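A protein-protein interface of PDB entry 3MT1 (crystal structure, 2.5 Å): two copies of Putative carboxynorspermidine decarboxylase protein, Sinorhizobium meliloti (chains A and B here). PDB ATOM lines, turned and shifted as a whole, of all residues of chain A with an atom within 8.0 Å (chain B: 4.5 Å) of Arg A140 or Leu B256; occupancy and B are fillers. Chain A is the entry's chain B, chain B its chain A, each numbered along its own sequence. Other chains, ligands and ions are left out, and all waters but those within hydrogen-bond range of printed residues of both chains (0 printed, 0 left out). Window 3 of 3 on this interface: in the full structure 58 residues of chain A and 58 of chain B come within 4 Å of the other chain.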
ATOM      1  N   TYR A  77      17.476 -22.362 -20.364  1.00  0.00           N
ATOM      2  CA  TYR A  77      18.589 -22.304 -19.436  1.00  0.00           C
ATOM      3  C   TYR A  77      18.353 -23.311 -18.331  1.00  0.00           C
ATOM      4  O   TYR A  77      17.204 -23.636 -18.002  1.00  0.00           O
ATOM      5  CB  TYR A  77      18.713 -20.917 -18.816  1.00  0.00           C
ATOM      6  CG  TYR A  77      19.744 -20.855 -17.697  1.00  0.00           C
ATOM      7  CD1 TYR A  77      21.105 -21.022 -17.959  1.00  0.00           C
ATOM      8  CD2 TYR A  77      19.347 -20.644 -16.365  1.00  0.00           C
ATOM      9  CE1 TYR A  77      22.049 -20.965 -16.945  1.00  0.00           C
ATOM     10  CE2 TYR A  77      20.276 -20.599 -15.337  1.00  0.00           C
ATOM     11  CZ  TYR A  77      21.634 -20.757 -15.628  1.00  0.00           C
ATOM     12  OH  TYR A  77      22.564 -20.699 -14.590  1.00  0.00           O
ATOM     13  N   VAL A  79      20.535 -24.770 -14.519  1.00  0.00           N
ATOM     14  CA  VAL A  79      21.705 -24.933 -13.683  1.00  0.00           C
ATOM     15  C   VAL A  79      22.312 -26.307 -13.964  1.00  0.00           C
ATOM     16  O   VAL A  79      23.523 -26.426 -14.078  1.00  0.00           O
ATOM     17  CB  VAL A  79      21.340 -24.744 -12.202  1.00  0.00           C
ATOM     18  CG1 VAL A  79      22.485 -25.030 -11.341  1.00  0.00           C
ATOM     19  CG2 VAL A  79      20.916 -23.318 -11.964  1.00  0.00           C
ATOM     20  N   ALA A  80      21.474 -27.321 -14.151  1.00  0.00           N
ATOM     21  CA  ALA A  80      21.957 -28.671 -14.468  1.00  0.00           C
ATOM     22  C   ALA A  80      20.977 -29.445 -15.352  1.00  0.00           C
ATOM     23  O   ALA A  80      19.887 -29.803 -14.866  1.00  0.00           O
ATOM     24  CB  ALA A  80      22.196 -29.437 -13.181  1.00  0.00           C
ATOM     25  N   ASN A  99      25.330 -23.608 -17.877  1.00  0.00           N
ATOM     26  CA  ASN A  99      25.818 -22.957 -16.677  1.00  0.00           C
ATOM     27  C   ASN A  99      27.338 -23.005 -16.544  1.00  0.00           C
ATOM     28  O   ASN A  99      27.939 -22.171 -15.870  1.00  0.00           O
ATOM     29  CB  ASN A  99      25.159 -23.594 -15.452  1.00  0.00           C
ATOM     30  CG  ASN A  99      25.281 -22.731 -14.213  1.00  0.00           C
ATOM     31  OD1 ASN A  99      24.729 -21.631 -14.164  1.00  0.00           O
ATOM     32  ND2 ASN A  99      26.005 -23.224 -13.203  1.00  0.00           N
ATOM     33  N   SER A 100      27.954 -23.978 -17.196  1.00  0.00           N
ATOM     34  CA  SER A 100      29.352 -24.293 -16.943  1.00  0.00           C
ATOM     35  C   SER A 100      29.918 -24.970 -18.168  1.00  0.00           C
ATOM     36  O   SER A 100      29.162 -25.504 -18.992  1.00  0.00           O
ATOM     37  CB  SER A 100      29.464 -25.234 -15.742  1.00  0.00           C
ATOM     38  OG  SER A 100      28.901 -26.495 -16.075  1.00  0.00           O
ATOM     39  N   ARG A 119      26.755 -19.273 -19.747  1.00  0.00           N
ATOM     40  CA  ARG A 119      26.586 -18.213 -18.760  1.00  0.00           C
ATOM     41  C   ARG A 119      27.917 -17.724 -18.216  1.00  0.00           C
ATOM     42  O   ARG A 119      28.803 -18.511 -17.871  1.00  0.00           O
ATOM     43  CB  ARG A 119      25.729 -18.674 -17.595  1.00  0.00           C
ATOM     44  CG  ARG A 119      25.315 -17.532 -16.717  1.00  0.00           C
ATOM     45  CD  ARG A 119      24.519 -17.984 -15.545  1.00  0.00           C
ATOM     46  NE  ARG A 119      24.068 -16.838 -14.761  1.00  0.00           N
ATOM     47  CZ  ARG A 119      23.087 -16.880 -13.867  1.00  0.00           C
ATOM     48  NH1 ARG A 119      22.434 -18.025 -13.642  1.00  0.00           N
ATOM     49  NH2 ARG A 119      22.753 -15.775 -13.209  1.00  0.00           N
ATOM     50  N   ASN A 121      29.776 -15.267 -15.318  1.00  0.00           N
ATOM     51  CA  ASN A 121      29.571 -14.720 -13.987  1.00  0.00           C
ATOM     52  C   ASN A 121      30.455 -13.498 -13.859  1.00  0.00           C
ATOM     53  O   ASN A 121      31.685 -13.625 -13.879  1.00  0.00           O
ATOM     54  CB  ASN A 121      29.944 -15.769 -12.940  1.00  0.00           C
ATOM     55  CG  ASN A 121      29.653 -15.324 -11.502  1.00  0.00           C
ATOM     56  OD1 ASN A 121      29.309 -14.169 -11.229  1.00  0.00           O
ATOM     57  ND2 ASN A 121      29.814 -16.259 -10.567  1.00  0.00           N
ATOM     58  N   ARG A 140      28.886 -20.116  -8.232  1.00  0.00           N
ATOM     59  CA  ARG A 140      28.326 -21.336  -8.823  1.00  0.00           C
ATOM     60  C   ARG A 140      27.312 -21.120  -9.985  1.00  0.00           C
ATOM     61  O   ARG A 140      26.635 -22.059 -10.432  1.00  0.00           O
ATOM     62  CB  ARG A 140      27.739 -22.256  -7.734  1.00  0.00           C
ATOM     63  CG  ARG A 140      26.422 -21.810  -7.098  1.00  0.00           C
ATOM     64  CD  ARG A 140      25.844 -22.922  -6.177  1.00  0.00           C
ATOM     65  NE  ARG A 140      24.433 -22.714  -5.827  1.00  0.00           N
ATOM     66  CZ  ARG A 140      23.398 -23.106  -6.576  1.00  0.00           C
ATOM     67  NH1 ARG A 140      23.599 -23.744  -7.726  1.00  0.00           N
ATOM     68  NH2 ARG A 140      22.152 -22.856  -6.181  1.00  0.00           N
ATOM     69  N   LEU A 141      27.207 -19.883 -10.456  1.00  0.00           N
ATOM     70  CA  LEU A 141      26.385 -19.570 -11.625  1.00  0.00           C
ATOM     71  C   LEU A 141      27.222 -18.861 -12.675  1.00  0.00           C
ATOM     72  O   LEU A 141      27.546 -17.689 -12.518  1.00  0.00           O
ATOM     73  CB  LEU A 141      25.210 -18.675 -11.247  1.00  0.00           C
ATOM     74  CG  LEU A 141      24.245 -19.129 -10.155  1.00  0.00           C
ATOM     75  CD1 LEU A 141      23.195 -18.054  -9.939  1.00  0.00           C
ATOM     76  CD2 LEU A 141      23.591 -20.473 -10.492  1.00  0.00           C
ATOM     77  N   GLY A 142      27.571 -19.573 -13.739  1.00  0.00           N
ATOM     78  CA  GLY A 142      28.368 -19.001 -14.819  1.00  0.00           C
ATOM     79  C   GLY A 142      29.870 -19.144 -14.629  1.00  0.00           C
ATOM     80  O   GLY A 142      30.361 -19.291 -13.510  1.00  0.00           O
ATOM     81  N   GLU A 143      30.599 -19.112 -15.735  1.00  0.00           N
ATOM     82  CA  GLU A 143      32.057 -19.176 -15.684  1.00  0.00           C
ATOM     83  C   GLU A 143      32.630 -17.761 -15.591  1.00  0.00           C
ATOM     84  O   GLU A 143      32.067 -16.833 -16.159  1.00  0.00           O
ATOM     85  CB  GLU A 143      32.612 -19.916 -16.906  1.00  0.00           C
ATOM     86  CG  GLU A 143      32.091 -21.357 -17.083  1.00  0.00           C
ATOM     87  CD  GLU A 143      32.747 -22.378 -16.143  1.00  0.00           C
ATOM     88  OE1 GLU A 143      33.767 -22.050 -15.499  1.00  0.00           O
ATOM     89  OE2 GLU A 143      32.247 -23.520 -16.058  1.00  0.00           O
ATOM     90  N   TRP A 144      33.730 -17.594 -14.860  1.00  0.00           N
ATOM     91  CA  TRP A 144      34.351 -16.286 -14.706  1.00  0.00           C
ATOM     92  C   TRP A 144      35.723 -16.270 -15.342  1.00  0.00           C
ATOM     93  O   TRP A 144      36.241 -15.203 -15.668  1.00  0.00           O
ATOM     94  CB  TRP A 144      34.481 -15.909 -13.222  1.00  0.00           C
ATOM     95  CG  TRP A 144      35.525 -16.705 -12.486  1.00  0.00           C
ATOM     96  CD1 TRP A 144      36.864 -16.431 -12.402  1.00  0.00           C
ATOM     97  CD2 TRP A 144      35.316 -17.909 -11.751  1.00  0.00           C
ATOM     98  NE1 TRP A 144      37.502 -17.394 -11.657  1.00  0.00           N
ATOM     99  CE2 TRP A 144      36.576 -18.314 -11.244  1.00  0.00           C
ATOM    100  CE3 TRP A 144      34.186 -18.691 -11.470  1.00  0.00           C
ATOM    101  CZ2 TRP A 144      36.737 -19.465 -10.463  1.00  0.00           C
ATOM    102  CZ3 TRP A 144      34.342 -19.841 -10.688  1.00  0.00           C
ATOM    103  CH2 TRP A 144      35.612 -20.215 -10.192  1.00  0.00           C
ATOM    104  N   ASP B 248      24.767 -33.050 -11.352  1.00  0.00           N
ATOM    105  CA  ASP B 248      25.937 -32.263 -11.612  1.00  0.00           C
ATOM    106  C   ASP B 248      26.690 -32.228 -10.311  1.00  0.00           C
ATOM    107  O   ASP B 248      26.112 -32.393  -9.248  1.00  0.00           O
ATOM    108  CB  ASP B 248      25.525 -30.853 -12.051  1.00  0.00           C
ATOM    109  CG  ASP B 248      26.677 -30.046 -12.628  1.00  0.00           C
ATOM    110  OD1 ASP B 248      27.553 -30.623 -13.306  1.00  0.00           O
ATOM    111  OD2 ASP B 248      26.702 -28.814 -12.414  1.00  0.00           O
ATOM    112  N   THR B 249      27.996 -32.055 -10.412  1.00  0.00           N
ATOM    113  CA  THR B 249      28.875 -31.988  -9.251  1.00  0.00           C
ATOM    114  C   THR B 249      30.011 -30.996  -9.520  1.00  0.00           C
ATOM    115  O   THR B 249      30.472 -30.910 -10.652  1.00  0.00           O
ATOM    116  CB  THR B 249      29.393 -33.387  -8.814  1.00  0.00           C
ATOM    117  OG1 THR B 249      30.148 -33.239  -7.610  1.00  0.00           O
ATOM    118  CG2 THR B 249      30.249 -34.070  -9.889  1.00  0.00           C
ATOM    119  N   LEU B 250      30.418 -30.221  -8.507  1.00  0.00           N
ATOM    120  CA  LEU B 250      31.369 -29.119  -8.714  1.00  0.00           C
ATOM    121  C   LEU B 250      32.037 -28.622  -7.420  1.00  0.00           C
ATOM    122  O   LEU B 250      31.633 -29.003  -6.322  1.00  0.00           O
ATOM    123  CB  LEU B 250      30.681 -27.973  -9.467  1.00  0.00           C
ATOM    124  CG  LEU B 250      30.020 -26.849  -8.667  1.00  0.00           C
ATOM    125  CD1 LEU B 250      30.823 -25.550  -8.866  1.00  0.00           C
ATOM    126  CD2 LEU B 250      28.548 -26.666  -9.085  1.00  0.00           C
ATOM    127  N   LYS B 254      33.352 -25.473  -1.627  1.00  0.00           N
ATOM    128  CA  LYS B 254      33.030 -26.751  -1.036  1.00  0.00           C
ATOM    129  C   LYS B 254      32.749 -27.736  -2.169  1.00  0.00           C
ATOM    130  O   LYS B 254      32.559 -27.322  -3.312  1.00  0.00           O
ATOM    131  CB  LYS B 254      31.811 -26.602  -0.110  1.00  0.00           C
ATOM    132  N   ASN B 255      32.775 -29.032  -1.869  1.00  0.00           N
ATOM    133  CA  ASN B 255      32.269 -30.029  -2.805  1.00  0.00           C
ATOM    134  C   ASN B 255      30.760 -29.809  -2.955  1.00  0.00           C
ATOM    135  O   ASN B 255      30.050 -29.747  -1.955  1.00  0.00           O
ATOM    136  CB  ASN B 255      32.571 -31.457  -2.317  1.00  0.00           C
ATOM    137  CG  ASN B 255      33.982 -31.953  -2.725  1.00  0.00           C
ATOM    138  OD1 ASN B 255      34.295 -32.067  -3.912  1.00  0.00           O
ATOM    139  ND2 ASN B 255      34.815 -32.267  -1.738  1.00  0.00           N
ATOM    140  N   LEU B 256      30.286 -29.656  -4.196  1.00  0.00           N
ATOM    141  CA  LEU B 256      28.864 -29.425  -4.471  1.00  0.00           C
ATOM    142  C   LEU B 256      28.231 -30.548  -5.276  1.00  0.00           C
ATOM    143  O   LEU B 256      28.882 -31.177  -6.096  1.00  0.00           O
ATOM    144  CB  LEU B 256      28.633 -28.080  -5.182  1.00  0.00           C
ATOM    145  CG  LEU B 256      28.852 -26.801  -4.367  1.00  0.00           C
ATOM    146  CD1 LEU B 256      28.147 -25.648  -5.035  1.00  0.00           C
ATOM    147  CD2 LEU B 256      28.306 -26.948  -2.954  1.00  0.00           C
ATOM    148  N   ALA B 257      26.962 -30.817  -5.011  1.00  0.00           N
ATOM    149  CA  ALA B 257      26.191 -31.703  -5.856  1.00  0.00           C
ATOM    150  C   ALA B 257      24.812 -31.103  -6.054  1.00  0.00           C
ATOM    151  O   ALA B 257      24.204 -30.630  -5.113  1.00  0.00           O
ATOM    152  CB  ALA B 257      26.108 -33.105  -5.262  1.00  0.00           C
ATOM    153  N   ILE B 258      24.350 -31.100  -7.296  1.00  0.00           N
ATOM    154  CA  ILE B 258      23.033 -30.606  -7.628  1.00  0.00           C
ATOM    155  C   ILE B 258      22.154 -31.785  -7.974  1.00  0.00           C
ATOM    156  O   ILE B 258      22.565 -32.685  -8.715  1.00  0.00           O
ATOM    157  CB  ILE B 258      23.090 -29.616  -8.819  1.00  0.00           C
ATOM    158  CG1 ILE B 258      24.204 -28.592  -8.553  1.00  0.00           C
ATOM    159  CG2 ILE B 258      21.684 -28.982  -9.055  1.00  0.00           C
ATOM    160  CD1 ILE B 258      24.131 -27.337  -9.408  1.00  0.00           C
ATOM    161  N   TYR B 288      29.738 -33.267   0.811  1.00  0.00           N
ATOM    162  CA  TYR B 288      29.233 -32.426  -0.264  1.00  0.00           C
ATOM    163  C   TYR B 288      28.115 -31.593   0.297  1.00  0.00           C
ATOM    164  O   TYR B 288      27.359 -32.059   1.140  1.00  0.00           O
ATOM    165  CB  TYR B 288      28.632 -33.258  -1.383  1.00  0.00           C
ATOM    166  CG  TYR B 288      29.595 -33.978  -2.281  1.00  0.00           C
ATOM    167  CD1 TYR B 288      29.837 -33.520  -3.575  1.00  0.00           C
ATOM    168  CD2 TYR B 288      30.231 -35.146  -1.859  1.00  0.00           C
ATOM    169  CE1 TYR B 288      30.717 -34.191  -4.422  1.00  0.00           C
ATOM    170  CE2 TYR B 288      31.094 -35.826  -2.697  1.00  0.00           C
ATOM    171  CZ  TYR B 288      31.332 -35.345  -3.975  1.00  0.00           C
ATOM    172  OH  TYR B 288      32.187 -36.034  -4.806  1.00  0.00           O
ATOM    173  N   MET B 289      28.009 -30.363  -0.170  1.00  0.00           N
ATOM    174  CA  MET B 289      26.852 -29.552   0.119  1.00  0.00           C
ATOM    175  C   MET B 289      25.863 -29.762  -1.013  1.00  0.00           C
ATOM    176  O   MET B 289      26.231 -29.614  -2.199  1.00  0.00           O
ATOM    177  CB  MET B 289      27.216 -28.088   0.213  1.00  0.00           C
ATOM    178  CG  MET B 289      26.013 -27.236   0.471  1.00  0.00           C
ATOM    179  SD  MET B 289      26.321 -25.424  -0.094  1.00  0.00           S
ATOM    180  CE  MET B 289      27.207 -24.749   1.549  1.00  0.00           C
ATOM    181  N   CYS B 291      22.419 -29.185  -3.317  1.00  0.00           N
ATOM    182  CA  CYS B 291      21.586 -28.070  -3.796  1.00  0.00           C
ATOM    183  C   CYS B 291      20.556 -28.469  -4.792  1.00  0.00           C
ATOM    184  O   CYS B 291      20.725 -29.428  -5.552  1.00  0.00           O
ATOM    185  CB  CYS B 291      22.416 -27.014  -4.526  1.00  0.00           C
ATOM    186  SG  CYS B 291      23.927 -26.666  -3.791  1.00  0.00           S
ATOM    187  N   SER B 294      17.881 -25.216  -8.952  1.00  0.00           N
ATOM    188  CA  SER B 294      17.592 -23.828  -9.292  1.00  0.00           C
ATOM    189  C   SER B 294      18.737 -22.942  -8.871  1.00  0.00           C
ATOM    190  O   SER B 294      19.716 -23.414  -8.268  1.00  0.00           O
ATOM    191  CB  SER B 294      16.324 -23.336  -8.620  1.00  0.00           C
ATOM    192  OG  SER B 294      16.652 -22.652  -7.407  1.00  0.00           O
ATOM    193  N   CYS B 295      18.614 -21.648  -9.162  1.00  0.00           N
ATOM    194  CA  CYS B 295      19.738 -20.723  -8.930  1.00  0.00           C
ATOM    195  C   CYS B 295      19.545 -19.715  -7.797  1.00  0.00           C
ATOM    196  O   CYS B 295      20.022 -18.586  -7.870  1.00  0.00           O
ATOM    197  CB  CYS B 295      20.168 -20.025 -10.232  1.00  0.00           C
ATOM    198  SG  CYS B 295      18.845 -19.288 -11.193  1.00  0.00           S
ATOM    199  N   LEU B 296      18.871 -20.147  -6.739  1.00  0.00           N
ATOM    200  CA  LEU B 296      18.668 -19.308  -5.568  1.00  0.00           C
ATOM    201  C   LEU B 296      19.766 -19.447  -4.508  1.00  0.00           C
ATOM    202  O   LEU B 296      20.313 -20.537  -4.305  1.00  0.00           O
ATOM    203  CB  LEU B 296      17.328 -19.632  -4.959  1.00  0.00           C
ATOM    204  CG  LEU B 296      16.164 -18.849  -5.540  1.00  0.00           C
ATOM    205  CD1 LEU B 296      16.115 -18.876  -7.084  1.00  0.00           C
ATOM    206  CD2 LEU B 296      14.905 -19.431  -4.895  1.00  0.00           C
ATOM    207  N   ASP B 299      18.663 -22.129  -2.041  1.00  0.00           N
ATOM    208  CA  ASP B 299      18.326 -23.494  -2.540  1.00  0.00           C
ATOM    209  C   ASP B 299      19.326 -24.609  -2.197  1.00  0.00           C
ATOM    210  O   ASP B 299      20.104 -25.057  -3.038  1.00  0.00           O
ATOM    211  CB  ASP B 299      18.040 -23.491  -4.048  1.00  0.00           C
ATOM    212  CG  ASP B 299      17.245 -24.753  -4.520  1.00  0.00           C
ATOM    213  OD1 ASP B 299      17.003 -25.691  -3.704  1.00  0.00           O
ATOM    214  OD2 ASP B 299      16.866 -24.789  -5.723  1.00  0.00           O
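O of Ser B294 is in hydrogen-bond range of NH2 of Arg A140.
O of Asp B248 lies within hydrogen-bond range of N of Ile B258 (2.9 Å). OG1 of Thr B249 is in hydrogen-bond range of O of Leu B256 (2.9 Å). The side-chain hydroxyl (OG) of Ser B294 sits at hydrogen-bond distance from the backbone NH (N) of Leu B296, 3.4 Å away. OG of Ser B294 sits at hydrogen-bond distance from OD2 of Asp B299 (2.7 Å). The side-chain amide nitrogen of Asn A99 is in hydrogen-bond range of the backbone carbonyl oxygen of Arg A140. The side-chain amide nitrogen (ND2) of Asn A121 lies close to the backbone carbonyl oxygen (O) of Leu A141, at 3.3 Å.
No position is printed for both chains.
Of the printed residues of chain B, Arg A140 touches Leu B256, Ser B294 and Leu B296. Leu B256 touches just one residue of chain A: Arg A140. Of the printed residues of chain B, Leu A141 touches Cys B295 (3.5 Å). Of the printed residues of chain A, Leu B296 touches Arg A140. Printed residues of chain B within 4 Å of Val A79: Ile B258 (3.4 Å), Ser B294 (3.8 Å) and Cys B295 (3.8 Å). Of the printed residues of chain A, Ser B294 touches Val A79 and Arg A140. Cys B291 touches none of the printed residues of chain A. The nearest printed residue of chain B that does not touch Arg A140 is Ile B258 (4.003 Å). The nearest printed residue of chain A that does not touch Ile B258 is Arg A140 (4.003 Å).
Among the printed residues, pairs that only touch across the chains: Val A79 with Ile B258 (3.4 Å), Leu A141 with Cys B295 (3.5 Å), Arg A140 with Leu B296 (3.5 Å), Arg A140 with Leu B256 (3.7 Å), Ala A80 with Asp B248 (3.8 Å), Val A79 with Cys B295 (3.8 Å) and Val A79 with Ser B294 (3.8 Å).
Hydrophobic or aromatic side chains of chain A that line the printed part of chain B: Val A79, Ala A80 and Leu A141. Among the printed residues, 8 pairs touch across the chains. Among the printed residues, no Asp or Glu carboxylate lies within 4 Å of a Lys or Arg side-chain nitrogen of the other chain.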
